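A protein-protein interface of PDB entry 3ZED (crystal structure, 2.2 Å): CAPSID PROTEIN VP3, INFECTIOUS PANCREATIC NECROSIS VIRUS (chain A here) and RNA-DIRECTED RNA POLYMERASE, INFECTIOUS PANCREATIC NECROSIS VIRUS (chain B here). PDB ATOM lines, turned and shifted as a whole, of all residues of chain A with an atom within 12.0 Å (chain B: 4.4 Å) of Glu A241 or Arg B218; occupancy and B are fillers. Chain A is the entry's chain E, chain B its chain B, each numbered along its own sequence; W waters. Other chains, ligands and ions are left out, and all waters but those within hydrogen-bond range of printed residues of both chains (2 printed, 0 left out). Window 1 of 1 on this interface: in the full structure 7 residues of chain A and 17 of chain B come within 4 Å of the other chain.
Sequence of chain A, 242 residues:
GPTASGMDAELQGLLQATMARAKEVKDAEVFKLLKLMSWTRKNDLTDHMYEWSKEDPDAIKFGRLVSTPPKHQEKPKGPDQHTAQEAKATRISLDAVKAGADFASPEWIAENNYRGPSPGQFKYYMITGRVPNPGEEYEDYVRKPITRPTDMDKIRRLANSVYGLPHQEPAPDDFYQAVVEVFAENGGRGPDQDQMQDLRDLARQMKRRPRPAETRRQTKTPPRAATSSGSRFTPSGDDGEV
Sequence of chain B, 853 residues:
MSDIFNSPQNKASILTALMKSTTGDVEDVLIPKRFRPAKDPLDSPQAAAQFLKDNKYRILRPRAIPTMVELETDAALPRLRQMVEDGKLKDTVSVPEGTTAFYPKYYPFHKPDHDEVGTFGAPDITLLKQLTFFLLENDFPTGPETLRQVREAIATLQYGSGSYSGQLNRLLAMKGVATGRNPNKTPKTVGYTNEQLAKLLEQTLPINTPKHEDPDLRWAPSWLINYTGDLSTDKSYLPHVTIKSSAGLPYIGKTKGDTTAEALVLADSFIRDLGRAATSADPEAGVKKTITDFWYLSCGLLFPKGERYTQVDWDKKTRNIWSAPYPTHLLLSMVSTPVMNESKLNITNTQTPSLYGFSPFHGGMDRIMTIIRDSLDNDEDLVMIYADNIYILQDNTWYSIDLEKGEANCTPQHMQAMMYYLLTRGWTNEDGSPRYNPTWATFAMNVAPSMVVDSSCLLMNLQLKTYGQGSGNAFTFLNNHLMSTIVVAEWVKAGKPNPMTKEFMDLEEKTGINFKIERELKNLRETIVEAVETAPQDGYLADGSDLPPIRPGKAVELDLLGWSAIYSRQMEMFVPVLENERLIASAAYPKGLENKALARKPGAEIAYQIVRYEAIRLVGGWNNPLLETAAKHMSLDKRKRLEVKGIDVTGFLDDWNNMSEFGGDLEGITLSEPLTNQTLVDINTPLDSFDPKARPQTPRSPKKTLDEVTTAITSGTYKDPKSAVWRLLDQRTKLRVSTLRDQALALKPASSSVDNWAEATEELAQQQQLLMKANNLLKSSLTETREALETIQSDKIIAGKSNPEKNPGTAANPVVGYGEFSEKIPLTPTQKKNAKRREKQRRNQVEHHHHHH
The guanidinium group (NH1) of Arg A232 is in salt-bridge range of the side-chain carboxylate (OD1) of Asp B216. OE2 of Glu A241 is in salt-bridge range of NH1 of Arg B218. The backbone NH (N) of Val A242 sits at hydrogen-bond distance from the backbone carbonyl oxygen (O) of Arg B218, 2.8 Å away. ND2 of Asn B437 sits at hydrogen-bond distance from OE2 of Glu A241 (3.1 Å). The chain-end carboxylate of Val A242 is in hydrogen-bond range of the side-chain amide nitrogen of Asn B437.
NE of Arg B218 lies within salt-bridge range of OD2 of Asp B216 (2.9 Å). O of Leu B217 lies within hydrogen-bond range of N of Asn B437. ND2 of Asn B437 lies within hydrogen-bond range of O of Arg B218, 3.1 Å away. O of Ser B751 sits at hydrogen-bond distance from NH1 of Arg B218 (2.7 Å). The backbone carbonyl oxygen (O) of Trp B219 sits at hydrogen-bond distance from the indole nitrogen (NE1) of Trp B440 (3.1 Å). The side-chain amide oxygen (OD1) of Asn B437 sits at hydrogen-bond distance from the backbone NH (N) of Trp B440, at 3.1 Å.
CE2 of Trp B219 touches CD of Pro A235 (3.6 Å). O of Gly A240 touches CD1 of Trp B219, 3.9 Å away. Glu A241 touches Trp B219. C of Trp B219 touches CG2 of Val A242 (3.7 Å). Trp B440 touches Val A242.
Of the printed residues of chain B, Arg A232 touches Asp B216. Thr A234 touches none of the printed residues of chain B. Of the printed residues of chain B, Pro A235 touches Trp B219. Glu A241 touches three residues of chain B. Of the printed residues of chain B, Val A242 touches Arg B218, Trp B219, Asn B437 and Trp B440. Asp B216 touches one residue of chain A. Arg B218 touches two residues of chain A. Of chain A, only Pro A235, Gly A240, Glu A241 and Val A242 come within 4 Å of Trp B219. Asn B437 touches two residues of chain A. Printed residues of chain A within 4 Å of Trp B440: Val A242 (3.6 Å). No residue of chain A comes within 4 Å of Ser B751. The nearest printed residue of chain B that does not touch Glu A241 is Ser B751 (5.1 Å). The nearest residue of chain A that does not touch Arg B218 is Gly A240 (5.3 Å). The nearest printed residue of chain A that does not touch Trp B440 is Glu A241 (7.1 Å).
Of the 7 printed residues of chain A, 5 touch a printed residue of chain B. Printed residues of chain A that touch a printed residue of chain B: Arg A232, Pro A235, Gly A240, Glu A241 and Val A242. Hydrophobic or aromatic side chains of chain A that line the printed part of chain B: Pro A235 and Val A242. Along chain A the printed residues that touch a printed residue of chain B span positions 232 to 242. Among the printed residues, Asp or Glu carboxylates within 4 Å of a Lys or Arg side-chain nitrogen of the other chain: Arg A232 with Asp B216 (3.1 Å) and Glu A241 with Arg B218 (3.5 Å).
Water W2 bridges OXT of Val A242 (2.7 Å) and ND2 of Asn B437 (3.2 Å). Water W1 lies within hydrogen-bond range of the backbone carbonyl oxygen (O) of Phe A233 (2.7 Å) and the backbone NH (N) of Asp B216 (2.9 Å).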
ATOM      1  N   ARG A 232      20.312  25.058  10.608  1.00  0.00           N
ATOM      2  CA  ARG A 232      20.411  23.804   9.836  1.00  0.00           C
ATOM      3  C   ARG A 232      19.953  24.042   8.409  1.00  0.00           C
ATOM      4  O   ARG A 232      18.883  24.632   8.208  1.00  0.00           O
ATOM      5  CB  ARG A 232      19.601  22.646  10.459  1.00  0.00           C
ATOM      6  CG  ARG A 232      19.725  21.310   9.658  1.00  0.00           C
ATOM      7  CD  ARG A 232      19.294  20.065  10.420  1.00  0.00           C
ATOM      8  NE  ARG A 232      19.936  19.969  11.736  1.00  0.00           N
ATOM      9  CZ  ARG A 232      19.464  19.267  12.763  1.00  0.00           C
ATOM     10  NH1 ARG A 232      18.348  18.559  12.634  1.00  0.00           N
ATOM     11  NH2 ARG A 232      20.101  19.276  13.932  1.00  0.00           N
ATOM     12  N   PHE A 233      20.725  23.551   7.416  1.00  0.00           N
ATOM     13  CA  PHE A 233      20.335  23.734   6.025  1.00  0.00           C
ATOM     14  C   PHE A 233      19.075  22.927   5.711  1.00  0.00           C
ATOM     15  O   PHE A 233      19.024  21.718   5.947  1.00  0.00           O
ATOM     16  CB  PHE A 233      21.477  23.398   5.060  1.00  0.00           C
ATOM     17  CG  PHE A 233      21.139  23.589   3.599  1.00  0.00           C
ATOM     18  CD1 PHE A 233      21.079  24.861   3.043  1.00  0.00           C
ATOM     19  CD2 PHE A 233      20.906  22.497   2.777  1.00  0.00           C
ATOM     20  CE1 PHE A 233      20.779  25.035   1.689  1.00  0.00           C
ATOM     21  CE2 PHE A 233      20.596  22.672   1.425  1.00  0.00           C
ATOM     22  CZ  PHE A 233      20.538  23.941   0.888  1.00  0.00           C
ATOM     23  N   THR A 234      18.034  23.643   5.258  1.00  0.00           N
ATOM     24  CA  THR A 234      16.744  23.091   4.858  1.00  0.00           C
ATOM     25  C   THR A 234      16.400  23.717   3.495  1.00  0.00           C
ATOM     26  O   THR A 234      16.015  24.891   3.462  1.00  0.00           O
ATOM     27  CB  THR A 234      15.643  23.326   5.935  1.00  0.00           C
ATOM     28  OG1 THR A 234      15.306  24.716   5.982  1.00  0.00           O
ATOM     29  CG2 THR A 234      16.025  22.811   7.336  1.00  0.00           C
ATOM     30  N   PRO A 235      16.578  23.003   2.360  1.00  0.00           N
ATOM     31  CA  PRO A 235      16.259  23.614   1.050  1.00  0.00           C
ATOM     32  C   PRO A 235      14.766  23.946   0.887  1.00  0.00           C
ATOM     33  O   PRO A 235      14.377  24.693  -0.012  1.00  0.00           O
ATOM     34  CB  PRO A 235      16.687  22.545   0.043  1.00  0.00           C
ATOM     35  CG  PRO A 235      16.658  21.263   0.812  1.00  0.00           C
ATOM     36  CD  PRO A 235      17.064  21.617   2.207  1.00  0.00           C
ATOM     37  N   GLY A 240       8.567  19.580   0.329  1.00  0.00           N
ATOM     38  CA  GLY A 240       9.623  19.446  -0.672  1.00  0.00           C
ATOM     39  C   GLY A 240      10.541  18.247  -0.486  1.00  0.00           C
ATOM     40  O   GLY A 240      11.274  17.882  -1.413  1.00  0.00           O
ATOM     41  N   GLU A 241      10.502  17.617   0.708  1.00  0.00           N
ATOM     42  CA  GLU A 241      11.345  16.477   1.013  1.00  0.00           C
ATOM     43  C   GLU A 241      10.902  15.202   0.263  1.00  0.00           C
ATOM     44  O   GLU A 241       9.731  15.074  -0.096  1.00  0.00           O
ATOM     45  CB  GLU A 241      11.512  16.244   2.524  1.00  0.00           C
ATOM     46  CG  GLU A 241      10.326  15.961   3.420  1.00  0.00           C
ATOM     47  CD  GLU A 241      10.740  15.949   4.884  1.00  0.00           C
ATOM     48  OE1 GLU A 241      11.270  16.981   5.352  1.00  0.00           O
ATOM     49  OE2 GLU A 241      10.605  14.892   5.540  1.00  0.00           O
ATOM     50  N   VAL A 242      11.867  14.301  -0.053  1.00  0.00           N
ATOM     51  CA  VAL A 242      11.574  13.073  -0.799  1.00  0.00           C
ATOM     52  C   VAL A 242      10.868  12.025   0.101  1.00  0.00           C
ATOM     53  O   VAL A 242      10.134  11.164  -0.453  1.00  0.00           O
ATOM     54  CB  VAL A 242      12.819  12.474  -1.512  1.00  0.00           C
ATOM     55  CG1 VAL A 242      13.271  13.370  -2.664  1.00  0.00           C
ATOM     56  CG2 VAL A 242      13.965  12.192  -0.531  1.00  0.00           C
ATOM     57  OXT VAL A 242      10.978  12.115   1.346  1.00  0.00           O
ATOM     58  N   ASP B 216      19.567  17.096   7.116  1.00  0.00           N
ATOM     59  CA  ASP B 216      19.047  15.796   7.484  1.00  0.00           C
ATOM     60  C   ASP B 216      18.860  14.954   6.233  1.00  0.00           C
ATOM     61  O   ASP B 216      18.817  15.497   5.122  1.00  0.00           O
ATOM     62  CB  ASP B 216      17.694  15.968   8.191  1.00  0.00           C
ATOM     63  CG  ASP B 216      17.698  16.645   9.545  1.00  0.00           C
ATOM     64  OD1 ASP B 216      18.778  16.744  10.159  1.00  0.00           O
ATOM     65  OD2 ASP B 216      16.611  17.024  10.015  1.00  0.00           O
ATOM     66  N   LEU B 217      18.709  13.640   6.402  1.00  0.00           N
ATOM     67  CA  LEU B 217      18.444  12.733   5.293  1.00  0.00           C
ATOM     68  C   LEU B 217      16.968  12.845   4.899  1.00  0.00           C
ATOM     69  O   LEU B 217      16.147  12.046   5.338  1.00  0.00           O
ATOM     70  CB  LEU B 217      18.819  11.289   5.700  1.00  0.00           C
ATOM     71  CG  LEU B 217      20.289  11.035   5.994  1.00  0.00           C
ATOM     72  CD1 LEU B 217      20.492   9.635   6.592  1.00  0.00           C
ATOM     73  CD2 LEU B 217      21.144  11.309   4.762  1.00  0.00           C
ATOM     74  N   ARG B 218      16.609  13.887   4.132  1.00  0.00           N
ATOM     75  CA  ARG B 218      15.213  14.109   3.764  1.00  0.00           C
ATOM     76  C   ARG B 218      15.020  14.506   2.314  1.00  0.00           C
ATOM     77  O   ARG B 218      13.871  14.603   1.869  1.00  0.00           O
ATOM     78  CB  ARG B 218      14.584  15.231   4.631  1.00  0.00           C
ATOM     79  CG  ARG B 218      14.622  15.029   6.132  1.00  0.00           C
ATOM     80  CD  ARG B 218      14.284  16.326   6.852  1.00  0.00           C
ATOM     81  NE  ARG B 218      14.389  16.180   8.304  1.00  0.00           N
ATOM     82  CZ  ARG B 218      13.446  15.655   9.078  1.00  0.00           C
ATOM     83  NH1 ARG B 218      12.309  15.230   8.551  1.00  0.00           N
ATOM     84  NH2 ARG B 218      13.638  15.542  10.384  1.00  0.00           N
ATOM     85  N   TRP B 219      16.101  14.809   1.595  1.00  0.00           N
ATOM     86  CA  TRP B 219      15.967  15.362   0.257  1.00  0.00           C
ATOM     87  C   TRP B 219      16.687  14.608  -0.837  1.00  0.00           C
ATOM     88  O   TRP B 219      17.540  13.748  -0.576  1.00  0.00           O
ATOM     89  CB  TRP B 219      16.499  16.807   0.278  1.00  0.00           C
ATOM     90  CG  TRP B 219      15.682  17.717   1.153  1.00  0.00           C
ATOM     91  CD1 TRP B 219      14.480  18.291   0.848  1.00  0.00           C
ATOM     92  CD2 TRP B 219      15.961  18.063   2.514  1.00  0.00           C
ATOM     93  NE1 TRP B 219      14.020  19.025   1.919  1.00  0.00           N
ATOM     94  CE2 TRP B 219      14.901  18.887   2.962  1.00  0.00           C
ATOM     95  CE3 TRP B 219      17.007  17.752   3.404  1.00  0.00           C
ATOM     96  CZ2 TRP B 219      14.879  19.444   4.245  1.00  0.00           C
ATOM     97  CZ3 TRP B 219      16.973  18.289   4.681  1.00  0.00           C
ATOM     98  CH2 TRP B 219      15.922  19.123   5.090  1.00  0.00           C
ATOM     99  N   PRO B 434      14.356  11.779  14.909  1.00  0.00           N
ATOM    100  CA  PRO B 434      15.239  11.389  13.799  1.00  0.00           C
ATOM    101  C   PRO B 434      15.626  12.526  12.843  1.00  0.00           C
ATOM    102  O   PRO B 434      14.803  13.379  12.520  1.00  0.00           O
ATOM    103  CB  PRO B 434      14.415  10.328  13.069  1.00  0.00           C
ATOM    104  CG  PRO B 434      13.006  10.697  13.334  1.00  0.00           C
ATOM    105  CD  PRO B 434      12.996  11.235  14.726  1.00  0.00           C
ATOM    106  N   TYR B 436      16.120  12.212   9.734  1.00  0.00           N
ATOM    107  CA  TYR B 436      15.741  11.526   8.507  1.00  0.00           C
ATOM    108  C   TYR B 436      14.224  11.373   8.445  1.00  0.00           C
ATOM    109  O   TYR B 436      13.543  11.459   9.468  1.00  0.00           O
ATOM    110  CB  TYR B 436      16.440  10.148   8.390  1.00  0.00           C
ATOM    111  CG  TYR B 436      16.219   9.216   9.566  1.00  0.00           C
ATOM    112  CD1 TYR B 436      15.058   8.447   9.667  1.00  0.00           C
ATOM    113  CD2 TYR B 436      17.170   9.101  10.575  1.00  0.00           C
ATOM    114  CE1 TYR B 436      14.852   7.588  10.745  1.00  0.00           C
ATOM    115  CE2 TYR B 436      16.969   8.251  11.663  1.00  0.00           C
ATOM    116  CZ  TYR B 436      15.804   7.499  11.745  1.00  0.00           C
ATOM    117  OH  TYR B 436      15.605   6.664  12.816  1.00  0.00           O
ATOM    118  N   ASN B 437      13.703  11.140   7.235  1.00  0.00           N
ATOM    119  CA  ASN B 437      12.292  10.922   6.991  1.00  0.00           C
ATOM    120  C   ASN B 437      12.056   9.438   6.600  1.00  0.00           C
ATOM    121  O   ASN B 437      13.045   8.684   6.469  1.00  0.00           O
ATOM    122  CB  ASN B 437      11.777  11.910   5.919  1.00  0.00           C
ATOM    123  CG  ASN B 437      12.340  11.829   4.513  1.00  0.00           C
ATOM    124  OD1 ASN B 437      12.916  10.832   4.063  1.00  0.00           O
ATOM    125  ND2 ASN B 437      12.066  12.859   3.741  1.00  0.00           N
ATOM    126  N   TRP B 440      14.175   8.102   3.431  1.00  0.00           N
ATOM    127  CA  TRP B 440      15.591   7.831   3.664  1.00  0.00           C
ATOM    128  C   TRP B 440      15.800   6.634   4.607  1.00  0.00           C
ATOM    129  O   TRP B 440      16.785   5.916   4.437  1.00  0.00           O
ATOM    130  CB  TRP B 440      16.328   9.075   4.142  1.00  0.00           C
ATOM    131  CG  TRP B 440      16.820   9.886   2.983  1.00  0.00           C
ATOM    132  CD1 TRP B 440      16.160  10.901   2.347  1.00  0.00           C
ATOM    133  CD2 TRP B 440      18.033   9.671   2.249  1.00  0.00           C
ATOM    134  NE1 TRP B 440      16.928  11.385   1.310  1.00  0.00           N
ATOM    135  CE2 TRP B 440      18.084  10.647   1.228  1.00  0.00           C
ATOM    136  CE3 TRP B 440      19.097   8.760   2.372  1.00  0.00           C
ATOM    137  CZ2 TRP B 440      19.139  10.714   0.311  1.00  0.00           C
ATOM    138  CZ3 TRP B 440      20.165   8.859   1.494  1.00  0.00           C
ATOM    139  CH2 TRP B 440      20.178   9.822   0.474  1.00  0.00           C
ATOM    140  N   SER B 751       9.540  12.131  12.561  1.00  0.00           N
ATOM    141  CA  SER B 751      10.374  12.754  11.526  1.00  0.00           C
ATOM    142  C   SER B 751       9.889  14.186  11.195  1.00  0.00           C
ATOM    143  O   SER B 751      10.693  14.996  10.734  1.00  0.00           O
ATOM    144  CB  SER B 751      10.472  11.878  10.277  1.00  0.00           C
ATOM    145  OG  SER B 751       9.322  11.913   9.453  1.00  0.00           O
HETATM  146  O   HOH W   1      17.995  19.544   7.189  1.00  0.00           O
HETATM  147  O   HOH W   2       9.572  10.881   3.269  1.00  0.00           O
